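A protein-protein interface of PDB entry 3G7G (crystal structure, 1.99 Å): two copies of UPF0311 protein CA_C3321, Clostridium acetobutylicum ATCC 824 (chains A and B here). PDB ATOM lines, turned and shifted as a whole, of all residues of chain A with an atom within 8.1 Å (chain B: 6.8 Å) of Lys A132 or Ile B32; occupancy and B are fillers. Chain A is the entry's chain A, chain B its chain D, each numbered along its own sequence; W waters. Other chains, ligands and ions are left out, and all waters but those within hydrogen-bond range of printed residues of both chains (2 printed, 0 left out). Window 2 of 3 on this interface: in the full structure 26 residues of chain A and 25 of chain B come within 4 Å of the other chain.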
ATOM      1  N   PHE A 124      11.040 -28.596  10.625  1.00  0.00           N
ATOM      2  CA  PHE A 124      10.385 -28.805  11.896  1.00  0.00           C
ATOM      3  C   PHE A 124      10.130 -27.538  12.692  1.00  0.00           C
ATOM      4  O   PHE A 124      10.897 -26.587  12.630  1.00  0.00           O
ATOM      5  CB  PHE A 124      11.193 -29.749  12.769  1.00  0.00           C
ATOM      6  CG  PHE A 124      11.461 -31.080  12.134  1.00  0.00           C
ATOM      7  CD1 PHE A 124      10.483 -32.035  12.033  1.00  0.00           C
ATOM      8  CD2 PHE A 124      12.697 -31.357  11.595  1.00  0.00           C
ATOM      9  CE1 PHE A 124      10.768 -33.269  11.434  1.00  0.00           C
ATOM     10  CE2 PHE A 124      12.963 -32.560  11.024  1.00  0.00           C
ATOM     11  CZ  PHE A 124      12.016 -33.505  10.935  1.00  0.00           C
ATOM     12  N   GLU A 125       9.050 -27.568  13.467  1.00  0.00           N
ATOM     13  CA  GLU A 125       8.732 -26.523  14.426  1.00  0.00           C
ATOM     14  C   GLU A 125       8.486 -27.203  15.764  1.00  0.00           C
ATOM     15  O   GLU A 125       7.710 -28.110  15.829  1.00  0.00           O
ATOM     16  CB  GLU A 125       7.534 -25.735  13.936  1.00  0.00           C
ATOM     17  CG  GLU A 125       7.119 -24.649  14.841  1.00  0.00           C
ATOM     18  CD  GLU A 125       5.947 -23.940  14.349  1.00  0.00           C
ATOM     19  OE1 GLU A 125       4.835 -24.297  14.750  1.00  0.00           O
ATOM     20  OE2 GLU A 125       6.129 -23.016  13.552  1.00  0.00           O
ATOM     21  N   THR A 126       9.219 -26.804  16.803  1.00  0.00           N
ATOM     22  CA  THR A 126       9.195 -27.452  18.113  1.00  0.00           C
ATOM     23  C   THR A 126       9.009 -26.371  19.203  1.00  0.00           C
ATOM     24  O   THR A 126       9.193 -25.203  18.927  1.00  0.00           O
ATOM     25  CB  THR A 126      10.484 -28.226  18.364  1.00  0.00           C
ATOM     26  OG1 THR A 126      11.588 -27.327  18.331  1.00  0.00           O
ATOM     27  CG2 THR A 126      10.695 -29.273  17.293  1.00  0.00           C
ATOM     28  N   TYR A 127       8.613 -26.771  20.417  1.00  0.00           N
ATOM     29  CA  TYR A 127       8.150 -25.821  21.462  1.00  0.00           C
ATOM     30  C   TYR A 127       8.785 -26.085  22.817  1.00  0.00           C
ATOM     31  O   TYR A 127       8.217 -25.768  23.887  1.00  0.00           O
ATOM     32  CB  TYR A 127       6.613 -25.847  21.573  1.00  0.00           C
ATOM     33  CG  TYR A 127       5.994 -25.994  20.217  1.00  0.00           C
ATOM     34  CD1 TYR A 127       5.713 -24.879  19.446  1.00  0.00           C
ATOM     35  CD2 TYR A 127       5.771 -27.253  19.661  1.00  0.00           C
ATOM     36  CE1 TYR A 127       5.194 -25.010  18.169  1.00  0.00           C
ATOM     37  CE2 TYR A 127       5.230 -27.388  18.392  1.00  0.00           C
ATOM     38  CZ  TYR A 127       4.970 -26.253  17.638  1.00  0.00           C
ATOM     39  OH  TYR A 127       4.427 -26.352  16.356  1.00  0.00           O
ATOM     40  N   SER A 128       9.998 -26.607  22.767  1.00  0.00           N
ATOM     41  CA  SER A 128      10.691 -26.992  23.972  1.00  0.00           C
ATOM     42  C   SER A 128      12.158 -27.023  23.654  1.00  0.00           C
ATOM     43  O   SER A 128      12.507 -27.466  22.569  1.00  0.00           O
ATOM     44  CB  SER A 128      10.164 -28.364  24.379  1.00  0.00           C
ATOM     45  OG  SER A 128      11.130 -29.125  25.024  1.00  0.00           O
ATOM     46  N   PRO A 129      13.037 -26.516  24.562  1.00  0.00           N
ATOM     47  CA  PRO A 129      14.501 -26.637  24.407  1.00  0.00           C
ATOM     48  C   PRO A 129      15.071 -28.021  24.097  1.00  0.00           C
ATOM     49  O   PRO A 129      16.116 -28.121  23.483  1.00  0.00           O
ATOM     50  CB  PRO A 129      15.022 -26.178  25.785  1.00  0.00           C
ATOM     51  CG  PRO A 129      14.056 -25.143  26.171  1.00  0.00           C
ATOM     52  CD  PRO A 129      12.717 -25.727  25.768  1.00  0.00           C
ATOM     53  N   LYS A 130      14.397 -29.084  24.498  1.00  0.00           N
ATOM     54  CA  LYS A 130      14.900 -30.423  24.256  1.00  0.00           C
ATOM     55  C   LYS A 130      14.895 -30.700  22.760  1.00  0.00           C
ATOM     56  O   LYS A 130      15.748 -31.426  22.282  1.00  0.00           O
ATOM     57  CB  LYS A 130      14.048 -31.444  24.985  1.00  0.00           C
ATOM     58  CG  LYS A 130      14.592 -32.822  24.998  1.00  0.00           C
ATOM     59  CD  LYS A 130      13.614 -33.785  25.587  1.00  0.00           C
ATOM     60  CE  LYS A 130      14.225 -35.200  25.654  1.00  0.00           C
ATOM     61  NZ  LYS A 130      13.170 -36.208  26.023  1.00  0.00           N
ATOM     62  N   TYR A 131      13.955 -30.107  22.033  1.00  0.00           N
ATOM     63  CA  TYR A 131      13.828 -30.353  20.578  1.00  0.00           C
ATOM     64  C   TYR A 131      14.151 -29.150  19.679  1.00  0.00           C
ATOM     65  O   TYR A 131      13.892 -29.219  18.456  1.00  0.00           O
ATOM     66  CB  TYR A 131      12.416 -30.880  20.255  1.00  0.00           C
ATOM     67  CG  TYR A 131      12.118 -32.115  21.066  1.00  0.00           C
ATOM     68  CD1 TYR A 131      12.657 -33.349  20.709  1.00  0.00           C
ATOM     69  CD2 TYR A 131      11.344 -32.040  22.224  1.00  0.00           C
ATOM     70  CE1 TYR A 131      12.421 -34.467  21.474  1.00  0.00           C
ATOM     71  CE2 TYR A 131      11.125 -33.135  22.989  1.00  0.00           C
ATOM     72  CZ  TYR A 131      11.662 -34.346  22.606  1.00  0.00           C
ATOM     73  OH  TYR A 131      11.408 -35.441  23.359  1.00  0.00           O
ATOM     74  N   LYS A 132      14.767 -28.092  20.223  1.00  0.00           N
ATOM     75  CA  LYS A 132      15.047 -26.923  19.384  1.00  0.00           C
ATOM     76  C   LYS A 132      16.120 -27.194  18.285  1.00  0.00           C
ATOM     77  O   LYS A 132      16.153 -26.504  17.239  1.00  0.00           O
ATOM     78  CB  LYS A 132      15.336 -25.679  20.222  1.00  0.00           C
ATOM     79  CG  LYS A 132      14.065 -25.082  20.858  1.00  0.00           C
ATOM     80  CD  LYS A 132      13.127 -24.396  19.829  1.00  0.00           C
ATOM     81  CE  LYS A 132      11.828 -23.980  20.479  1.00  0.00           C
ATOM     82  NZ  LYS A 132      10.921 -23.062  19.659  1.00  0.00           N
ATOM     83  N   TRP A 133      16.951 -28.218  18.517  1.00  0.00           N
ATOM     84  CA  TRP A 133      17.937 -28.661  17.552  1.00  0.00           C
ATOM     85  C   TRP A 133      17.308 -29.062  16.216  1.00  0.00           C
ATOM     86  O   TRP A 133      17.959 -28.970  15.184  1.00  0.00           O
ATOM     87  CB  TRP A 133      18.758 -29.827  18.107  1.00  0.00           C
ATOM     88  CG  TRP A 133      17.989 -31.104  18.350  1.00  0.00           C
ATOM     89  CD1 TRP A 133      17.338 -31.481  19.509  1.00  0.00           C
ATOM     90  CD2 TRP A 133      17.818 -32.189  17.432  1.00  0.00           C
ATOM     91  NE1 TRP A 133      16.741 -32.719  19.339  1.00  0.00           N
ATOM     92  CE2 TRP A 133      17.029 -33.179  18.083  1.00  0.00           C
ATOM     93  CE3 TRP A 133      18.228 -32.415  16.107  1.00  0.00           C
ATOM     94  CZ2 TRP A 133      16.658 -34.377  17.451  1.00  0.00           C
ATOM     95  CZ3 TRP A 133      17.858 -33.610  15.489  1.00  0.00           C
ATOM     96  CH2 TRP A 133      17.090 -34.571  16.159  1.00  0.00           C
ATOM     97  N   MET A 134      16.032 -29.456  16.240  1.00  0.00           N
ATOM     98  CA  MET A 134      15.328 -29.863  15.039  1.00  0.00           C
ATOM     99  C   MET A 134      15.062 -28.653  14.162  1.00  0.00           C
ATOM    100  O   MET A 134      14.821 -28.785  12.957  1.00  0.00           O
ATOM    101  CB  MET A 134      14.016 -30.593  15.374  1.00  0.00           C
ATOM    102  CG  MET A 134      14.194 -31.885  16.180  1.00  0.00           C
ATOM    103  SD  MET A 134      12.685 -32.858  16.422  1.00  0.00           S
ATOM    104  CE  MET A 134      12.619 -33.564  14.811  1.00  0.00           C
ATOM    105  N   MET A 135      15.064 -27.468  14.766  1.00  0.00           N
ATOM    106  CA  MET A 135      14.932 -26.228  14.002  1.00  0.00           C
ATOM    107  C   MET A 135      16.303 -25.678  13.539  1.00  0.00           C
ATOM    108  O   MET A 135      16.376 -24.703  12.788  1.00  0.00           O
ATOM    109  CB  MET A 135      14.119 -25.185  14.795  1.00  0.00           C
ATOM    110  CG  MET A 135      12.709 -25.667  15.288  1.00  0.00           C
ATOM    111  SD  MET A 135      11.751 -24.382  16.152  1.00  0.00           S
ATOM    112  CE  MET A 135      11.451 -23.279  14.793  1.00  0.00           C
ATOM    113  N   ASN A 136      17.395 -26.318  13.936  1.00  0.00           N
ATOM    114  CA  ASN A 136      18.705 -25.747  13.654  1.00  0.00           C
ATOM    115  C   ASN A 136      19.652 -26.700  12.972  1.00  0.00           C
ATOM    116  O   ASN A 136      20.876 -26.535  13.014  1.00  0.00           O
ATOM    117  CB  ASN A 136      19.282 -25.171  14.952  1.00  0.00           C
ATOM    118  CG  ASN A 136      18.531 -23.943  15.407  1.00  0.00           C
ATOM    119  OD1 ASN A 136      18.668 -22.867  14.824  1.00  0.00           O
ATOM    120  ND2 ASN A 136      17.706 -24.098  16.406  1.00  0.00           N
ATOM    121  N   HIS A 137      19.068 -27.680  12.297  1.00  0.00           N
ATOM    122  CA  HIS A 137      19.799 -28.569  11.418  1.00  0.00           C
ATOM    123  C   HIS A 137      19.035 -28.756  10.107  1.00  0.00           C
ATOM    124  O   HIS A 137      17.794 -28.522  10.031  1.00  0.00           O
ATOM    125  CB  HIS A 137      19.968 -29.925  12.051  1.00  0.00           C
ATOM    126  CG  HIS A 137      20.849 -29.925  13.245  1.00  0.00           C
ATOM    127  ND1 HIS A 137      22.154 -30.368  13.204  1.00  0.00           N
ATOM    128  CD2 HIS A 137      20.621 -29.524  14.515  1.00  0.00           C
ATOM    129  CE1 HIS A 137      22.681 -30.260  14.411  1.00  0.00           C
ATOM    130  NE2 HIS A 137      21.775 -29.742  15.222  1.00  0.00           N
ATOM    131  N   PHE A 139      17.885 -31.582   7.318  1.00  0.00           N
ATOM    132  CA  PHE A 139      17.435 -32.966   7.327  1.00  0.00           C
ATOM    133  C   PHE A 139      17.020 -33.423   5.932  1.00  0.00           C
ATOM    134  O   PHE A 139      16.577 -32.632   5.091  1.00  0.00           O
ATOM    135  CB  PHE A 139      16.179 -33.114   8.193  1.00  0.00           C
ATOM    136  CG  PHE A 139      16.403 -32.897   9.651  1.00  0.00           C
ATOM    137  CD1 PHE A 139      16.522 -33.970  10.513  1.00  0.00           C
ATOM    138  CD2 PHE A 139      16.458 -31.623  10.160  1.00  0.00           C
ATOM    139  CE1 PHE A 139      16.698 -33.772  11.849  1.00  0.00           C
ATOM    140  CE2 PHE A 139      16.638 -31.408  11.501  1.00  0.00           C
ATOM    141  CZ  PHE A 139      16.778 -32.489  12.346  1.00  0.00           C
ATOM    142  N   GLN B  29       2.792 -24.736  21.756  1.00  0.00           N
ATOM    143  CA  GLN B  29       3.049 -23.292  21.900  1.00  0.00           C
ATOM    144  C   GLN B  29       4.304 -23.058  22.737  1.00  0.00           C
ATOM    145  O   GLN B  29       4.620 -23.854  23.626  1.00  0.00           O
ATOM    146  CB  GLN B  29       1.845 -22.621  22.600  1.00  0.00           C
ATOM    147  CG  GLN B  29       2.032 -21.186  23.033  1.00  0.00           C
ATOM    148  CD  GLN B  29       0.780 -20.578  23.699  1.00  0.00           C
ATOM    149  OE1 GLN B  29      -0.343 -20.938  23.356  1.00  0.00           O
ATOM    150  NE2 GLN B  29       0.987 -19.681  24.681  1.00  0.00           N
ATOM    151  N   ASP B  30       4.992 -21.958  22.461  1.00  0.00           N
ATOM    152  CA  ASP B  30       6.019 -21.436  23.346  1.00  0.00           C
ATOM    153  C   ASP B  30       6.105 -19.945  23.115  1.00  0.00           C
ATOM    154  O   ASP B  30       5.373 -19.397  22.290  1.00  0.00           O
ATOM    155  CB  ASP B  30       7.387 -22.170  23.217  1.00  0.00           C
ATOM    156  CG  ASP B  30       8.201 -21.789  21.974  1.00  0.00           C
ATOM    157  OD1 ASP B  30       7.840 -20.863  21.220  1.00  0.00           O
ATOM    158  OD2 ASP B  30       9.236 -22.457  21.740  1.00  0.00           O
ATOM    159  N   ASP B  31       6.966 -19.274  23.862  1.00  0.00           N
ATOM    160  CA  ASP B  31       7.034 -17.820  23.805  1.00  0.00           C
ATOM    161  C   ASP B  31       8.019 -17.245  22.748  1.00  0.00           C
ATOM    162  O   ASP B  31       8.225 -16.029  22.746  1.00  0.00           O
ATOM    163  CB  ASP B  31       7.342 -17.251  25.215  1.00  0.00           C
ATOM    164  CG  ASP B  31       6.098 -17.048  26.099  1.00  0.00           C
ATOM    165  OD1 ASP B  31       4.929 -17.199  25.654  1.00  0.00           O
ATOM    166  OD2 ASP B  31       6.304 -16.665  27.285  1.00  0.00           O
ATOM    167  N   ILE B  32       8.619 -18.046  21.853  1.00  0.00           N
ATOM    168  CA  ILE B  32       9.301 -17.446  20.652  1.00  0.00           C
ATOM    169  C   ILE B  32       8.601 -17.764  19.352  1.00  0.00           C
ATOM    170  O   ILE B  32       8.459 -16.875  18.522  1.00  0.00           O
ATOM    171  CB  ILE B  32      10.785 -17.908  20.318  1.00  0.00           C
ATOM    172  CG1 ILE B  32      11.304 -18.925  21.277  1.00  0.00           C
ATOM    173  CG2 ILE B  32      11.743 -16.706  20.033  1.00  0.00           C
ATOM    174  CD1 ILE B  32      10.989 -20.261  20.814  1.00  0.00           C
ATOM    175  N   VAL B  33       8.239 -19.026  19.120  1.00  0.00           N
ATOM    176  CA  VAL B  33       7.585 -19.396  17.835  1.00  0.00           C
ATOM    177  C   VAL B  33       6.108 -19.059  17.883  1.00  0.00           C
ATOM    178  O   VAL B  33       5.529 -18.654  16.876  1.00  0.00           O
ATOM    179  CB  VAL B  33       7.794 -20.865  17.411  1.00  0.00           C
ATOM    180  CG1 VAL B  33       9.288 -21.232  17.420  1.00  0.00           C
ATOM    181  CG2 VAL B  33       7.069 -21.784  18.266  1.00  0.00           C
ATOM    182  N   GLY B  34       5.494 -19.200  19.059  1.00  0.00           N
ATOM    183  CA  GLY B  34       4.080 -18.899  19.212  1.00  0.00           C
ATOM    184  C   GLY B  34       3.274 -20.162  19.279  1.00  0.00           C
ATOM    185  O   GLY B  34       3.821 -21.222  19.636  1.00  0.00           O
ATOM    186  N   ARG B  66       1.708 -15.682  16.729  1.00  0.00           N
ATOM    187  CA  ARG B  66       3.050 -15.321  17.148  1.00  0.00           C
ATOM    188  C   ARG B  66       2.972 -14.713  18.554  1.00  0.00           C
ATOM    189  O   ARG B  66       1.899 -14.290  18.994  1.00  0.00           O
ATOM    190  CB  ARG B  66       3.684 -14.363  16.143  1.00  0.00           C
ATOM    191  CG  ARG B  66       3.939 -14.969  14.755  1.00  0.00           C
ATOM    192  CD  ARG B  66       4.941 -16.113  14.865  1.00  0.00           C
ATOM    193  NE  ARG B  66       5.247 -16.667  13.564  1.00  0.00           N
ATOM    194  CZ  ARG B  66       6.012 -17.721  13.370  1.00  0.00           C
ATOM    195  NH1 ARG B  66       6.583 -18.340  14.386  1.00  0.00           N
ATOM    196  NH2 ARG B  66       6.231 -18.135  12.136  1.00  0.00           N
ATOM    197  N   PRO B  67       4.070 -14.766  19.308  1.00  0.00           N
ATOM    198  CA  PRO B  67       4.044 -14.204  20.651  1.00  0.00           C
ATOM    199  C   PRO B  67       3.546 -12.767  20.728  1.00  0.00           C
ATOM    200  O   PRO B  67       2.951 -12.402  21.736  1.00  0.00           O
ATOM    201  CB  PRO B  67       5.505 -14.310  21.084  1.00  0.00           C
ATOM    202  CG  PRO B  67       5.968 -15.543  20.401  1.00  0.00           C
ATOM    203  CD  PRO B  67       5.364 -15.407  19.032  1.00  0.00           C
HETATM  204  O   HOH W   1      10.847 -23.320  23.572  1.00  0.00           O
HETATM  205  O   HOH W   2       7.721 -20.930  13.297  1.00  0.00           O
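Among the printed residues, pairs that only touch across the chains: Lys A132 with Ile B32, Lys A132 with Val B33, Tyr A127 with Gln B29, Tyr A127 with Asp B30, Tyr A127 with Val B33, Thr A126 with Asp B30 and Met A135 with Val B33.
The side-chain hydroxyl of Tyr A127 lies within hydrogen-bond range of the side-chain carboxylate of Glu A125 (2.6 Å).
The backbone carbonyl oxygen (O) of Thr A126 is in hydrogen-bond range of the side-chain amino group (NZ) of Lys A132 (2.8 Å).
N of Thr A126 is in hydrogen-bond range of SD of Met A135, at 3.6 Å.
The backbone carbonyl oxygen of Lys A132 lies within hydrogen-bond range of the side-chain amide nitrogen of Asn A136.
OD1 of Asp B30 is in hydrogen-bond range of N of Ile B32 (3.0 Å).
OD1 of Asp B30 sits at hydrogen-bond distance from N of Val B33 (2.8 Å).
No position is printed for both chains.
Of the 8 pairs that touch across the chains among the printed residues, none has its exchanged pair printed and touching as well.
Water W1 bridges the side-chain carboxylate (OD2) of Asp B30 and the backbone NH (N) of Ser A128.
Water W2 bridges OE2 of Glu A125 (2.6 Å) and NH1 of Arg B66 (3.0 Å).
Printed residues of chain A within 4 Å of Asp B30: Thr A126 (3.9 Å), Tyr A127 (3.5 Å) and Lys A132 (2.7 Å).
Printed residues of chain B within 4 Å of Met A135: Val B33.
Of the printed residues of chain A, Val B33 touches Tyr A127 (3.6 Å), Lys A132 (3.3 Å) and Met A135 (3.97 Å).
The nearest residue of chain A that does not touch Ile B32 is Thr A126 (5.6 Å).
The nearest printed residue of chain B that does not touch Thr A126 is Val B33 (4.1 Å).
Of the 8 printed residues of chain B, 4 touch a printed residue of chain A.
Hydrophobic or aromatic side chains of chain B that line the printed part of chain A: Ile B32 and Val B33.
Along chain B the printed residues that touch a printed residue of chain A span positions 29 to 33.
Of the 15 printed residues of chain A, 4 touch a printed residue of chain B.
Hydrophobic or aromatic side chains of chain A that line the printed part of chain B: Tyr A127 and Met A135.
Among the printed residues, Asp or Glu carboxylates within 4 Å of a Lys or Arg side-chain nitrogen of the other chain: Lys A132 with Asp B30 (2.7 Å).
NZ of Lys A132 lies within salt-bridge range of OD2 of Asp B30 (2.7 Å).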
